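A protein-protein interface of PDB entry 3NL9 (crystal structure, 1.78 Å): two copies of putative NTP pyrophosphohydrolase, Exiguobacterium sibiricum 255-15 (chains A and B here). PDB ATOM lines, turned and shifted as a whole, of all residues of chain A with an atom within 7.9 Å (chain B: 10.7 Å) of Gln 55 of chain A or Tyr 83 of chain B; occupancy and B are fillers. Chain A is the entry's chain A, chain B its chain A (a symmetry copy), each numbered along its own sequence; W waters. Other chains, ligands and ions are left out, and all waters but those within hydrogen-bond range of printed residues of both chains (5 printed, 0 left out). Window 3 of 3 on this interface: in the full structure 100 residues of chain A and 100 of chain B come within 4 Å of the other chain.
A ring nitrogen (NE2) of His 51 of chain A is in hydrogen-bond range of the backbone carbonyl oxygen (O) of Glu 81 of chain B (2.9 Å). The side-chain amide nitrogen (NE2) of Gln 94 of chain B is in hydrogen-bond range of the side-chain hydroxyl (OG) of Ser 53 of chain A (2.8 Å). The backbone carbonyl oxygen (O) of Ser 78 of chain B lies within hydrogen-bond range of a ring nitrogen (NE2) of His 51 of chain A.
A ring nitrogen (ND1) of His 51 of chain A lies within hydrogen-bond range of the side-chain amide oxygen (OE1) of Gln 52 of chain A. The backbone carbonyl oxygen (O) of Ala 74 of chain B is in hydrogen-bond range of the side-chain hydroxyl (OG) of Ser 78 of chain B (3.2 Å). OD1 of Asn 56 of chain A is in hydrogen-bond range of N of Glu 59 of chain A (2.8 Å).
Among the printed residues, merely in contact across the chains: His 51 of chain A with Tyr 83 of chain B (3.2 Å), Gln 52 of chain A with Arg 90 of chain B (3.3 Å), His 51 of chain A with Thr 82 of chain B (3.3 Å), Gln 52 of chain A with Gly 93 of chain B (3.4 Å), Ser 54 of chain A with Pro 84 of chain B (3.4 Å), Phe 60 of chain A with Tyr 83 of chain B (3.4 Å), Gln 52 of chain A with Pro 84 of chain B (3.4 Å), Glu 57 of chain A with Tyr 83 of chain B (3.4 Å), Ser 54 of chain A with Tyr 83 of chain B (3.6 Å), Phe 60 of chain A with Leu 79 of chain B (3.6 Å), Glu 59 of chain A with Leu 31 of chain B (3.6 Å), Gln 55 of chain A with Tyr 83 of chain B (3.7 Å), Gln 55 of chain A with Arg 90 of chain B (3.7 Å), Leu 61 of chain A with Leu 79 of chain B (3.7 Å), Ser 54 of chain A with Leu 31 of chain B (3.7 Å), Asn 56 of chain A with Tyr 83 of chain B (3.8 Å), Ser 53 of chain A with Leu 31 of chain B (3.8 Å), His 51 of chain A with Pro 84 of chain B (3.8 Å), Ser 53 of chain A with Arg 90 of chain B (3.9 Å) and Gln 52 of chain A with Gln 94 of chain B (3.98 Å).
Of chain B, only Ser 78, Glu 81, Thr 82, Tyr 83 and Pro 84 come within 4 Å of His 51 of chain A. Of chain B, only Leu 31, Tyr 83 and Pro 84 come within 4 Å of Ser 54 of chain A. Of the printed residues of chain B, Gln 55 of chain A touches Tyr 83 (3.7 Å) and Arg 90 (3.7 Å). Glu 57 of chain A touches one residue of chain B. Of the printed residues of chain B, Glu 59 of chain A touches Leu 31. Of the printed residues of chain A, Ser 78 of chain B touches His 51. Of the printed residues of chain A, Leu 79 of chain B touches Phe 60 and Leu 61. Of the printed residues of chain A, Thr 82 of chain B touches His 51. Tyr 83 of chain B touches just these residues of chain A: His 51 (3.2 Å), Ser 54 (3.6 Å), Gln 55 (3.7 Å), Asn 56 (3.8 Å), Glu 57 (3.4 Å) and Phe 60 (3.4 Å). Of the printed residues of chain A, Pro 84 of chain B touches His 51 (3.8 Å), Gln 52 (3.4 Å) and Ser 54 (3.4 Å). The nearest residue of chain A that does not touch Tyr 83 of chain B is Gln 52 of chain A (5.6 Å). The nearest printed residue of chain A that does not touch Arg 90 of chain B is Ser 54 of chain A (4.6 Å).
Of the 25 printed residues of chain B, 10 touch a printed residue of chain A. Hydrophobic or aromatic side chains of chain B within 4 Å of the printed part of chain A: Leu 31, Leu 79, Tyr 83 and Pro 84.
No position is printed for both chains. Of the 23 pairs that touch across the chains among the printed residues, none has its exchanged pair printed and touching as well.
Water W5 bridges the backbone carbonyl oxygen (O) of Pro 84 of chain B (2.5 Å) and the backbone carbonyl oxygen (O) of Gln 55 of chain A (2.8 Å). Water W3 lies within hydrogen-bond range of O of Leu 79 of chain B (2.5 Å), OH of Tyr 83 of chain B (2.7 Å) and OE1 of Glu 57 of chain A (2.9 Å). Water W4 bridges NE2 of Gln 52 of chain A (2.7 Å) and O of Glu 89 of chain B (2.7 Å). Water W2 lies within hydrogen-bond range of O of Ile 29 of chain B and O of Ser 53 of chain A.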
ATOM      1  N   LEU A  50      23.615  24.622   9.837  1.00  0.00           N
ATOM      2  CA  LEU A  50      22.776  25.210  10.910  1.00  0.00           C
ATOM      3  C   LEU A  50      21.278  25.180  10.572  1.00  0.00           C
ATOM      4  O   LEU A  50      20.435  25.016  11.446  1.00  0.00           O
ATOM      5  CB  LEU A  50      23.263  26.635  11.275  1.00  0.00           C
ATOM      6  CG  LEU A  50      24.616  26.696  11.987  1.00  0.00           C
ATOM      7  CD1 LEU A  50      25.045  28.121  12.445  1.00  0.00           C
ATOM      8  CD2 LEU A  50      24.579  25.714  13.170  1.00  0.00           C
ATOM      9  N   HIS A  51      20.950  25.370   9.307  1.00  0.00           N
ATOM     10  CA  HIS A  51      19.562  25.324   8.881  1.00  0.00           C
ATOM     11  C   HIS A  51      19.068  23.898   9.060  1.00  0.00           C
ATOM     12  O   HIS A  51      17.999  23.677   9.618  1.00  0.00           O
ATOM     13  CB  HIS A  51      19.416  25.749   7.430  1.00  0.00           C
ATOM     14  CG  HIS A  51      18.009  25.690   6.916  1.00  0.00           C
ATOM     15  ND1 HIS A  51      17.429  24.525   6.458  1.00  0.00           N
ATOM     16  CD2 HIS A  51      17.069  26.657   6.770  1.00  0.00           C
ATOM     17  CE1 HIS A  51      16.196  24.777   6.056  1.00  0.00           C
ATOM     18  NE2 HIS A  51      15.953  26.063   6.235  1.00  0.00           N
ATOM     19  N   GLN A  52      19.871  22.926   8.614  1.00  0.00           N
ATOM     20  CA  GLN A  52      19.481  21.502   8.775  1.00  0.00           C
ATOM     21  C   GLN A  52      19.540  21.050  10.218  1.00  0.00           C
ATOM     22  O   GLN A  52      19.030  19.993  10.552  1.00  0.00           O
ATOM     23  CB  GLN A  52      20.335  20.616   7.903  1.00  0.00           C
ATOM     24  CG  GLN A  52      20.173  20.970   6.440  1.00  0.00           C
ATOM     25  CD  GLN A  52      18.787  20.668   5.943  1.00  0.00           C
ATOM     26  OE1 GLN A  52      17.954  21.567   5.744  1.00  0.00           O
ATOM     27  NE2 GLN A  52      18.519  19.406   5.772  1.00  0.00           N
ATOM     28  N   SER A  53      20.147  21.844  11.091  1.00  0.00           N
ATOM     29  CA  SER A  53      20.120  21.541  12.546  1.00  0.00           C
ATOM     30  C   SER A  53      18.912  22.186  13.270  1.00  0.00           C
ATOM     31  O   SER A  53      18.676  21.921  14.456  1.00  0.00           O
ATOM     32  CB  SER A  53      21.440  22.000  13.226  1.00  0.00           C
ATOM     33  OG  SER A  53      22.599  21.473  12.572  1.00  0.00           O
ATOM     34  N   SER A  54      18.173  23.045  12.568  1.00  0.00           N
ATOM     35  CA  SER A  54      17.096  23.842  13.145  1.00  0.00           C
ATOM     36  C   SER A  54      15.697  23.304  12.859  1.00  0.00           C
ATOM     37  O   SER A  54      15.454  22.703  11.826  1.00  0.00           O
ATOM     38  CB  SER A  54      17.175  25.277  12.597  1.00  0.00           C
ATOM     39  OG  SER A  54      18.337  25.936  13.072  1.00  0.00           O
ATOM     40  N   GLN A  55      14.761  23.563  13.763  1.00  0.00           N
ATOM     41  CA  GLN A  55      13.388  23.104  13.591  1.00  0.00           C
ATOM     42  C   GLN A  55      12.434  24.213  13.164  1.00  0.00           C
ATOM     43  O   GLN A  55      11.322  23.930  12.715  1.00  0.00           O
ATOM     44  CB  GLN A  55      12.902  22.407  14.862  1.00  0.00           C
ATOM     45  CG  GLN A  55      13.703  21.131  15.133  1.00  0.00           C
ATOM     46  CD  GLN A  55      13.365  20.471  16.456  1.00  0.00           C
ATOM     47  OE1 GLN A  55      12.287  19.895  16.613  1.00  0.00           O
ATOM     48  NE2 GLN A  55      14.294  20.534  17.408  1.00  0.00           N
ATOM     49  N   ASN A  56      12.877  25.466  13.260  1.00  0.00           N
ATOM     50  CA  ASN A  56      12.069  26.615  12.844  1.00  0.00           C
ATOM     51  C   ASN A  56      12.936  27.848  12.633  1.00  0.00           C
ATOM     52  O   ASN A  56      14.144  27.856  12.956  1.00  0.00           O
ATOM     53  CB  ASN A  56      10.968  26.914  13.882  1.00  0.00           C
ATOM     54  CG  ASN A  56      11.524  27.101  15.271  1.00  0.00           C
ATOM     55  OD1 ASN A  56      12.333  27.994  15.510  1.00  0.00           O
ATOM     56  ND2 ASN A  56      11.117  26.242  16.189  1.00  0.00           N
ATOM     57  N   GLU A  57      12.299  28.900  12.114  1.00  0.00           N
ATOM     58  CA  GLU A  57      12.992  30.150  11.777  1.00  0.00           C
ATOM     59  C   GLU A  57      13.593  30.801  13.028  1.00  0.00           C
ATOM     60  O   GLU A  57      14.701  31.310  12.989  1.00  0.00           O
ATOM     61  CB  GLU A  57      12.021  31.098  11.055  1.00  0.00           C
ATOM     62  CG  GLU A  57      12.608  32.443  10.696  1.00  0.00           C
ATOM     63  CD  GLU A  57      11.660  33.277   9.847  1.00  0.00           C
ATOM     64  OE1 GLU A  57      11.692  33.119   8.600  1.00  0.00           O
ATOM     65  OE2 GLU A  57      10.899  34.085  10.438  1.00  0.00           O
ATOM     66  N   THR A  58      12.864  30.758  14.135  1.00  0.00           N
ATOM     67  CA  THR A  58      13.327  31.379  15.387  1.00  0.00           C
ATOM     68  C   THR A  58      14.655  30.756  15.867  1.00  0.00           C
ATOM     69  O   THR A  58      15.620  31.485  16.173  1.00  0.00           O
ATOM     70  CB  THR A  58      12.244  31.288  16.458  1.00  0.00           C
ATOM     71  OG1 THR A  58      11.051  31.958  15.995  1.00  0.00           O
ATOM     72  CG2 THR A  58      12.707  31.914  17.782  1.00  0.00           C
ATOM     73  N   GLU A  59      14.704  29.419  15.907  1.00  0.00           N
ATOM     74  CA  GLU A  59      15.942  28.659  16.249  1.00  0.00           C
ATOM     75  C   GLU A  59      17.070  29.041  15.340  1.00  0.00           C
ATOM     76  O   GLU A  59      18.206  29.275  15.767  1.00  0.00           O
ATOM     77  CB  GLU A  59      15.736  27.134  16.082  1.00  0.00           C
ATOM     78  CG  GLU A  59      14.974  26.500  17.226  1.00  0.00           C
ATOM     79  CD  GLU A  59      15.174  25.006  17.359  1.00  0.00           C
ATOM     80  OE1 GLU A  59      15.526  24.296  16.373  1.00  0.00           O
ATOM     81  OE2 GLU A  59      14.962  24.532  18.491  1.00  0.00           O
ATOM     82  N   PHE A  60      16.757  29.035  14.052  1.00  0.00           N
ATOM     83  CA  PHE A  60      17.771  29.136  13.040  1.00  0.00           C
ATOM     84  C   PHE A  60      18.419  30.530  13.088  1.00  0.00           C
ATOM     85  O   PHE A  60      19.644  30.658  13.086  1.00  0.00           O
ATOM     86  CB  PHE A  60      17.163  28.820  11.681  1.00  0.00           C
ATOM     87  CG  PHE A  60      18.081  29.066  10.548  1.00  0.00           C
ATOM     88  CD1 PHE A  60      19.334  28.498  10.537  1.00  0.00           C
ATOM     89  CD2 PHE A  60      17.686  29.860   9.476  1.00  0.00           C
ATOM     90  CE1 PHE A  60      20.194  28.712   9.497  1.00  0.00           C
ATOM     91  CE2 PHE A  60      18.553  30.092   8.429  1.00  0.00           C
ATOM     92  CZ  PHE A  60      19.799  29.518   8.433  1.00  0.00           C
ATOM     93  N   LEU A  61      17.584  31.551  13.177  1.00  0.00           N
ATOM     94  CA  LEU A  61      18.060  32.915  13.274  1.00  0.00           C
ATOM     95  C   LEU A  61      18.881  33.146  14.556  1.00  0.00           C
ATOM     96  O   LEU A  61      19.920  33.828  14.508  1.00  0.00           O
ATOM     97  CB  LEU A  61      16.878  33.905  13.154  1.00  0.00           C
ATOM     98  CG  LEU A  61      16.295  34.046  11.749  1.00  0.00           C
ATOM     99  CD1 LEU A  61      15.206  35.131  11.680  1.00  0.00           C
ATOM    100  CD2 LEU A  61      17.444  34.294  10.756  1.00  0.00           C
ATOM    101  N   ALA B  28      21.843  12.974  15.277  1.00  0.00           N
ATOM    102  CA  ALA B  28      21.826  14.394  14.910  1.00  0.00           C
ATOM    103  C   ALA B  28      22.520  15.226  15.991  1.00  0.00           C
ATOM    104  O   ALA B  28      22.261  15.030  17.159  1.00  0.00           O
ATOM    105  CB  ALA B  28      20.375  14.912  14.716  1.00  0.00           C
ATOM    106  N   ILE B  29      23.350  16.174  15.587  1.00  0.00           N
ATOM    107  CA  ILE B  29      24.044  17.062  16.536  1.00  0.00           C
ATOM    108  C   ILE B  29      23.031  18.123  17.040  1.00  0.00           C
ATOM    109  O   ILE B  29      22.407  18.826  16.229  1.00  0.00           O
ATOM    110  CB  ILE B  29      25.276  17.739  15.873  1.00  0.00           C
ATOM    111  CG1 ILE B  29      26.306  16.704  15.434  1.00  0.00           C
ATOM    112  CG2 ILE B  29      25.950  18.725  16.847  1.00  0.00           C
ATOM    113  CD1 ILE B  29      27.368  17.274  14.508  1.00  0.00           C
ATOM    114  N   PRO B  30      22.827  18.229  18.375  1.00  0.00           N
ATOM    115  CA  PRO B  30      21.951  19.318  18.880  1.00  0.00           C
ATOM    116  C   PRO B  30      22.359  20.715  18.420  1.00  0.00           C
ATOM    117  O   PRO B  30      23.548  20.991  18.312  1.00  0.00           O
ATOM    118  CB  PRO B  30      22.102  19.212  20.402  1.00  0.00           C
ATOM    119  CG  PRO B  30      22.554  17.789  20.637  1.00  0.00           C
ATOM    120  CD  PRO B  30      23.449  17.487  19.484  1.00  0.00           C
ATOM    121  N   LEU B  31      21.369  21.592  18.193  1.00  0.00           N
ATOM    122  CA  LEU B  31      21.619  22.911  17.576  1.00  0.00           C
ATOM    123  C   LEU B  31      22.651  23.738  18.356  1.00  0.00           C
ATOM    124  O   LEU B  31      23.532  24.319  17.762  1.00  0.00           O
ATOM    125  CB  LEU B  31      20.311  23.700  17.372  1.00  0.00           C
ATOM    126  CG  LEU B  31      20.392  25.138  16.828  1.00  0.00           C
ATOM    127  CD1 LEU B  31      21.079  25.111  15.456  1.00  0.00           C
ATOM    128  CD2 LEU B  31      19.052  25.825  16.753  1.00  0.00           C
ATOM    129  N   ASP B  32      22.548  23.790  19.683  1.00  0.00           N
ATOM    130  CA  ASP B  32      23.476  24.629  20.454  1.00  0.00           C
ATOM    131  C   ASP B  32      24.911  24.143  20.346  1.00  0.00           C
ATOM    132  O   ASP B  32      25.824  24.941  20.310  1.00  0.00           O
ATOM    133  CB  ASP B  32      23.044  24.724  21.923  1.00  0.00           C
ATOM    134  CG  ASP B  32      21.801  25.593  22.112  1.00  0.00           C
ATOM    135  OD1 ASP B  32      21.565  26.516  21.293  1.00  0.00           O
ATOM    136  OD2 ASP B  32      21.062  25.346  23.086  1.00  0.00           O
ATOM    137  N   ALA B  74      23.315  33.666   1.732  1.00  0.00           N
ATOM    138  CA  ALA B  74      23.074  32.246   1.893  1.00  0.00           C
ATOM    139  C   ALA B  74      22.009  32.034   2.945  1.00  0.00           C
ATOM    140  O   ALA B  74      21.137  31.198   2.754  1.00  0.00           O
ATOM    141  CB  ALA B  74      24.377  31.485   2.253  1.00  0.00           C
ATOM    142  N   VAL B  75      22.076  32.784   4.051  1.00  0.00           N
ATOM    143  CA  VAL B  75      21.041  32.724   5.069  1.00  0.00           C
ATOM    144  C   VAL B  75      19.682  33.125   4.474  1.00  0.00           C
ATOM    145  O   VAL B  75      18.670  32.492   4.746  1.00  0.00           O
ATOM    146  CB  VAL B  75      21.353  33.647   6.263  1.00  0.00           C
ATOM    147  CG1 VAL B  75      20.206  33.613   7.270  1.00  0.00           C
ATOM    148  CG2 VAL B  75      22.656  33.239   6.958  1.00  0.00           C
ATOM    149  N   LYS B  76      19.653  34.189   3.671  1.00  0.00           N
ATOM    150  CA  LYS B  76      18.385  34.649   3.089  1.00  0.00           C
ATOM    151  C   LYS B  76      17.787  33.568   2.182  1.00  0.00           C
ATOM    152  O   LYS B  76      16.597  33.307   2.235  1.00  0.00           O
ATOM    153  CB  LYS B  76      18.574  35.971   2.321  1.00  0.00           C
ATOM    154  CG  LYS B  76      18.951  37.179   3.201  1.00  0.00           C
ATOM    155  CD  LYS B  76      19.101  38.459   2.381  1.00  0.00           C
ATOM    156  CE  LYS B  76      20.062  39.485   3.004  1.00  0.00           C
ATOM    157  NZ  LYS B  76      19.467  40.255   4.104  1.00  0.00           N
ATOM    158  N   LYS B  77      18.625  32.919   1.374  1.00  0.00           N
ATOM    159  CA  LYS B  77      18.169  31.797   0.570  1.00  0.00           C
ATOM    160  C   LYS B  77      17.650  30.657   1.451  1.00  0.00           C
ATOM    161  O   LYS B  77      16.585  30.099   1.172  1.00  0.00           O
ATOM    162  CB  LYS B  77      19.278  31.266  -0.342  1.00  0.00           C
ATOM    163  CG  LYS B  77      19.813  32.268  -1.386  1.00  0.00           C
ATOM    164  CD  LYS B  77      20.657  31.557  -2.468  1.00  0.00           C
ATOM    165  N   SER B  78      18.391  30.307   2.507  1.00  0.00           N
ATOM    166  CA  SER B  78      17.991  29.178   3.378  1.00  0.00           C
ATOM    167  C   SER B  78      16.702  29.434   4.177  1.00  0.00           C
ATOM    168  O   SER B  78      15.957  28.497   4.490  1.00  0.00           O
ATOM    169  CB  SER B  78      19.128  28.801   4.320  1.00  0.00           C
ATOM    170  OG  SER B  78      20.194  28.230   3.575  1.00  0.00           O
ATOM    171  N   LEU B  79      16.451  30.697   4.496  1.00  0.00           N
ATOM    172  CA  LEU B  79      15.238  31.097   5.222  1.00  0.00           C
ATOM    173  C   LEU B  79      13.963  30.728   4.445  1.00  0.00           C
ATOM    174  O   LEU B  79      12.894  30.581   5.038  1.00  0.00           O
ATOM    175  CB  LEU B  79      15.257  32.603   5.514  1.00  0.00           C
ATOM    176  CG  LEU B  79      16.172  33.088   6.644  1.00  0.00           C
ATOM    177  CD1 LEU B  79      16.193  34.651   6.711  1.00  0.00           C
ATOM    178  CD2 LEU B  79      15.743  32.491   7.985  1.00  0.00           C
ATOM    179  N   LYS B  80      14.091  30.572   3.126  1.00  0.00           N
ATOM    180  CA  LYS B  80      12.961  30.246   2.257  1.00  0.00           C
ATOM    181  C   LYS B  80      12.784  28.732   2.087  1.00  0.00           C
ATOM    182  O   LYS B  80      11.878  28.308   1.389  1.00  0.00           O
ATOM    183  CB  LYS B  80      13.147  30.910   0.881  1.00  0.00           C
ATOM    184  CG  LYS B  80      13.149  32.457   0.916  1.00  0.00           C
ATOM    185  CD  LYS B  80      13.746  33.075  -0.367  1.00  0.00           C
ATOM    186  CE  LYS B  80      13.551  34.601  -0.417  1.00  0.00           C
ATOM    187  N   GLU B  81      13.653  27.931   2.710  1.00  0.00           N
ATOM    188  CA  GLU B  81      13.616  26.468   2.594  1.00  0.00           C
ATOM    189  C   GLU B  81      13.012  25.900   3.859  1.00  0.00           C
ATOM    190  O   GLU B  81      13.331  26.378   4.944  1.00  0.00           O
ATOM    191  CB  GLU B  81      15.030  25.909   2.419  1.00  0.00           C
ATOM    192  CG  GLU B  81      15.697  26.288   1.100  1.00  0.00           C
ATOM    193  CD  GLU B  81      14.973  25.697  -0.120  1.00  0.00           C
ATOM    194  OE1 GLU B  81      14.747  24.457  -0.151  1.00  0.00           O
ATOM    195  OE2 GLU B  81      14.618  26.477  -1.040  1.00  0.00           O
ATOM    196  N   THR B  82      12.159  24.883   3.721  1.00  0.00           N
ATOM    197  CA  THR B  82      11.449  24.259   4.852  1.00  0.00           C
ATOM    198  C   THR B  82      12.443  23.549   5.780  1.00  0.00           C
ATOM    199  O   THR B  82      13.440  23.033   5.309  1.00  0.00           O
ATOM    200  CB  THR B  82      10.401  23.195   4.361  1.00  0.00           C
ATOM    201  OG1 THR B  82      11.082  22.202   3.600  1.00  0.00           O
ATOM    202  CG2 THR B  82       9.294  23.829   3.482  1.00  0.00           C
ATOM    203  N   TYR B  83      12.154  23.505   7.078  1.00  0.00           N
ATOM    204  CA  TYR B  83      13.107  22.985   8.072  1.00  0.00           C
ATOM    205  C   TYR B  83      12.876  21.484   8.216  1.00  0.00           C
ATOM    206  O   TYR B  83      11.787  21.005   7.954  1.00  0.00           O
ATOM    207  CB  TYR B  83      12.972  23.722   9.442  1.00  0.00           C
ATOM    208  CG  TYR B  83      13.352  25.171   9.331  1.00  0.00           C
ATOM    209  CD1 TYR B  83      14.675  25.568   9.444  1.00  0.00           C
ATOM    210  CD2 TYR B  83      12.392  26.138   9.052  1.00  0.00           C
ATOM    211  CE1 TYR B  83      15.037  26.897   9.283  1.00  0.00           C
ATOM    212  CE2 TYR B  83      12.736  27.474   8.890  1.00  0.00           C
ATOM    213  CZ  TYR B  83      14.075  27.844   9.006  1.00  0.00           C
ATOM    214  OH  TYR B  83      14.432  29.155   8.837  1.00  0.00           O
ATOM    215  N   PRO B  84      13.911  20.724   8.602  1.00  0.00           N
ATOM    216  CA  PRO B  84      13.674  19.328   8.938  1.00  0.00           C
ATOM    217  C   PRO B  84      12.562  19.153   9.979  1.00  0.00           C
ATOM    218  O   PRO B  84      12.428  19.975  10.882  1.00  0.00           O
ATOM    219  CB  PRO B  84      15.011  18.883   9.542  1.00  0.00           C
ATOM    220  CG  PRO B  84      15.990  19.822   9.038  1.00  0.00           C
ATOM    221  CD  PRO B  84      15.304  21.122   8.834  1.00  0.00           C
ATOM    222  N   VAL B  85      11.778  18.083   9.845  1.00  0.00           N
ATOM    223  CA  VAL B  85      10.684  17.780  10.777  1.00  0.00           C
ATOM    224  C   VAL B  85      10.932  16.512  11.611  1.00  0.00           C
ATOM    225  O   VAL B  85      10.133  16.194  12.493  1.00  0.00           O
ATOM    226  CB  VAL B  85       9.334  17.677  10.039  1.00  0.00           C
ATOM    227  CG1 VAL B  85       8.946  19.051   9.463  1.00  0.00           C
ATOM    228  CG2 VAL B  85       9.376  16.590   8.932  1.00  0.00           C
ATOM    229  N   THR B  86      12.021  15.785  11.339  1.00  0.00           N
ATOM    230  CA  THR B  86      12.430  14.655  12.188  1.00  0.00           C
ATOM    231  C   THR B  86      13.932  14.721  12.546  1.00  0.00           C
ATOM    232  O   THR B  86      14.725  15.397  11.887  1.00  0.00           O
ATOM    233  CB  THR B  86      12.150  13.276  11.505  1.00  0.00           C
ATOM    234  OG1 THR B  86      13.075  13.070  10.425  1.00  0.00           O
ATOM    235  CG2 THR B  86      10.695  13.176  10.976  1.00  0.00           C
ATOM    236  N   GLU B  87      14.324  13.958  13.558  1.00  0.00           N
ATOM    237  CA  GLU B  87      15.729  13.876  13.952  1.00  0.00           C
ATOM    238  C   GLU B  87      16.573  13.217  12.847  1.00  0.00           C
ATOM    239  O   GLU B  87      17.683  13.644  12.550  1.00  0.00           O
ATOM    240  CB  GLU B  87      15.824  13.112  15.265  1.00  0.00           C
ATOM    241  CG  GLU B  87      17.125  13.289  16.007  1.00  0.00           C
ATOM    242  CD  GLU B  87      17.126  12.557  17.353  1.00  0.00           C
ATOM    243  OE1 GLU B  87      16.053  12.521  18.012  1.00  0.00           O
ATOM    244  OE2 GLU B  87      18.199  12.021  17.741  1.00  0.00           O
ATOM    245  N   VAL B  88      16.008  12.220  12.173  1.00  0.00           N
ATOM    246  CA  VAL B  88      16.717  11.616  11.069  1.00  0.00           C
ATOM    247  C   VAL B  88      16.956  12.642   9.978  1.00  0.00           C
ATOM    248  O   VAL B  88      18.057  12.710   9.471  1.00  0.00           O
ATOM    249  CB  VAL B  88      15.991  10.397  10.491  1.00  0.00           C
ATOM    250  CG1 VAL B  88      16.662   9.993   9.175  1.00  0.00           C
ATOM    251  CG2 VAL B  88      16.045   9.266  11.499  1.00  0.00           C
ATOM    252  N   GLU B  89      15.940  13.445   9.643  1.00  0.00           N
ATOM    253  CA  GLU B  89      16.123  14.548   8.681  1.00  0.00           C
ATOM    254  C   GLU B  89      17.239  15.510   9.055  1.00  0.00           C
ATOM    255  O   GLU B  89      18.040  15.917   8.191  1.00  0.00           O
ATOM    256  CB  GLU B  89      14.820  15.327   8.456  1.00  0.00           C
ATOM    257  CG  GLU B  89      13.775  14.524   7.721  1.00  0.00           C
ATOM    258  CD  GLU B  89      12.547  15.317   7.314  1.00  0.00           C
ATOM    259  OE1 GLU B  89      12.476  16.540   7.561  1.00  0.00           O
ATOM    260  OE2 GLU B  89      11.655  14.690   6.717  1.00  0.00           O
ATOM    261  N   ARG B  90      17.306  15.888  10.324  1.00  0.00           N
ATOM    262  CA  ARG B  90      18.393  16.756  10.775  1.00  0.00           C
ATOM    263  C   ARG B  90      19.766  16.084  10.597  1.00  0.00           C
ATOM    264  O   ARG B  90      20.718  16.731  10.162  1.00  0.00           O
ATOM    265  CB  ARG B  90      18.154  17.217  12.229  1.00  0.00           C
ATOM    266  CG  ARG B  90      16.822  17.976  12.393  1.00  0.00           C
ATOM    267  CD  ARG B  90      16.608  18.681  13.750  1.00  0.00           C
ATOM    268  NE  ARG B  90      16.597  17.777  14.901  1.00  0.00           N
ATOM    269  CZ  ARG B  90      15.521  17.150  15.375  1.00  0.00           C
ATOM    270  NH1 ARG B  90      14.333  17.302  14.798  1.00  0.00           N
ATOM    271  NH2 ARG B  90      15.644  16.349  16.431  1.00  0.00           N
ATOM    272  N   LEU B  91      19.873  14.790  10.917  1.00  0.00           N
ATOM    273  CA  LEU B  91      21.160  14.066  10.764  1.00  0.00           C
ATOM    274  C   LEU B  91      21.585  14.000   9.301  1.00  0.00           C
ATOM    275  O   LEU B  91      22.748  14.234   8.941  1.00  0.00           O
ATOM    276  CB  LEU B  91      21.040  12.639  11.345  1.00  0.00           C
ATOM    277  CG  LEU B  91      22.244  11.693  11.270  1.00  0.00           C
ATOM    278  CD1 LEU B  91      23.455  12.266  12.062  1.00  0.00           C
ATOM    279  CD2 LEU B  91      21.843  10.293  11.753  1.00  0.00           C
ATOM    280  N   GLY B  93      20.706  15.975   6.818  1.00  0.00           N
ATOM    281  CA  GLY B  93      21.097  17.298   6.319  1.00  0.00           C
ATOM    282  C   GLY B  93      22.439  17.787   6.834  1.00  0.00           C
ATOM    283  O   GLY B  93      23.161  18.478   6.142  1.00  0.00           O
ATOM    284  N   GLN B  94      22.750  17.458   8.080  1.00  0.00           N
ATOM    285  CA  GLN B  94      24.061  17.742   8.650  1.00  0.00           C
ATOM    286  C   GLN B  94      25.166  16.980   7.914  1.00  0.00           C
ATOM    287  O   GLN B  94      26.190  17.564   7.517  1.00  0.00           O
ATOM    288  CB  GLN B  94      24.070  17.359  10.128  1.00  0.00           C
ATOM    289  CG  GLN B  94      23.366  18.343  10.993  1.00  0.00           C
ATOM    290  CD  GLN B  94      23.109  17.856  12.411  1.00  0.00           C
ATOM    291  OE1 GLN B  94      23.376  16.720  12.734  1.00  0.00           O
ATOM    292  NE2 GLN B  94      22.591  18.736  13.267  1.00  0.00           N
HETATM  293  O   HOH W   1      15.036  20.652   5.178  1.00  0.00           O
HETATM  294  O   HOH W   2      19.807  19.293  15.657  1.00  0.00           O
HETATM  295  O   HOH W   3      12.549  30.574   7.554  1.00  0.00           O
HETATM  296  O   HOH W   4      17.250  17.048   5.883  1.00  0.00           O
HETATM  297  O   HOH W   5      10.574  21.489  11.584  1.00  0.00           O
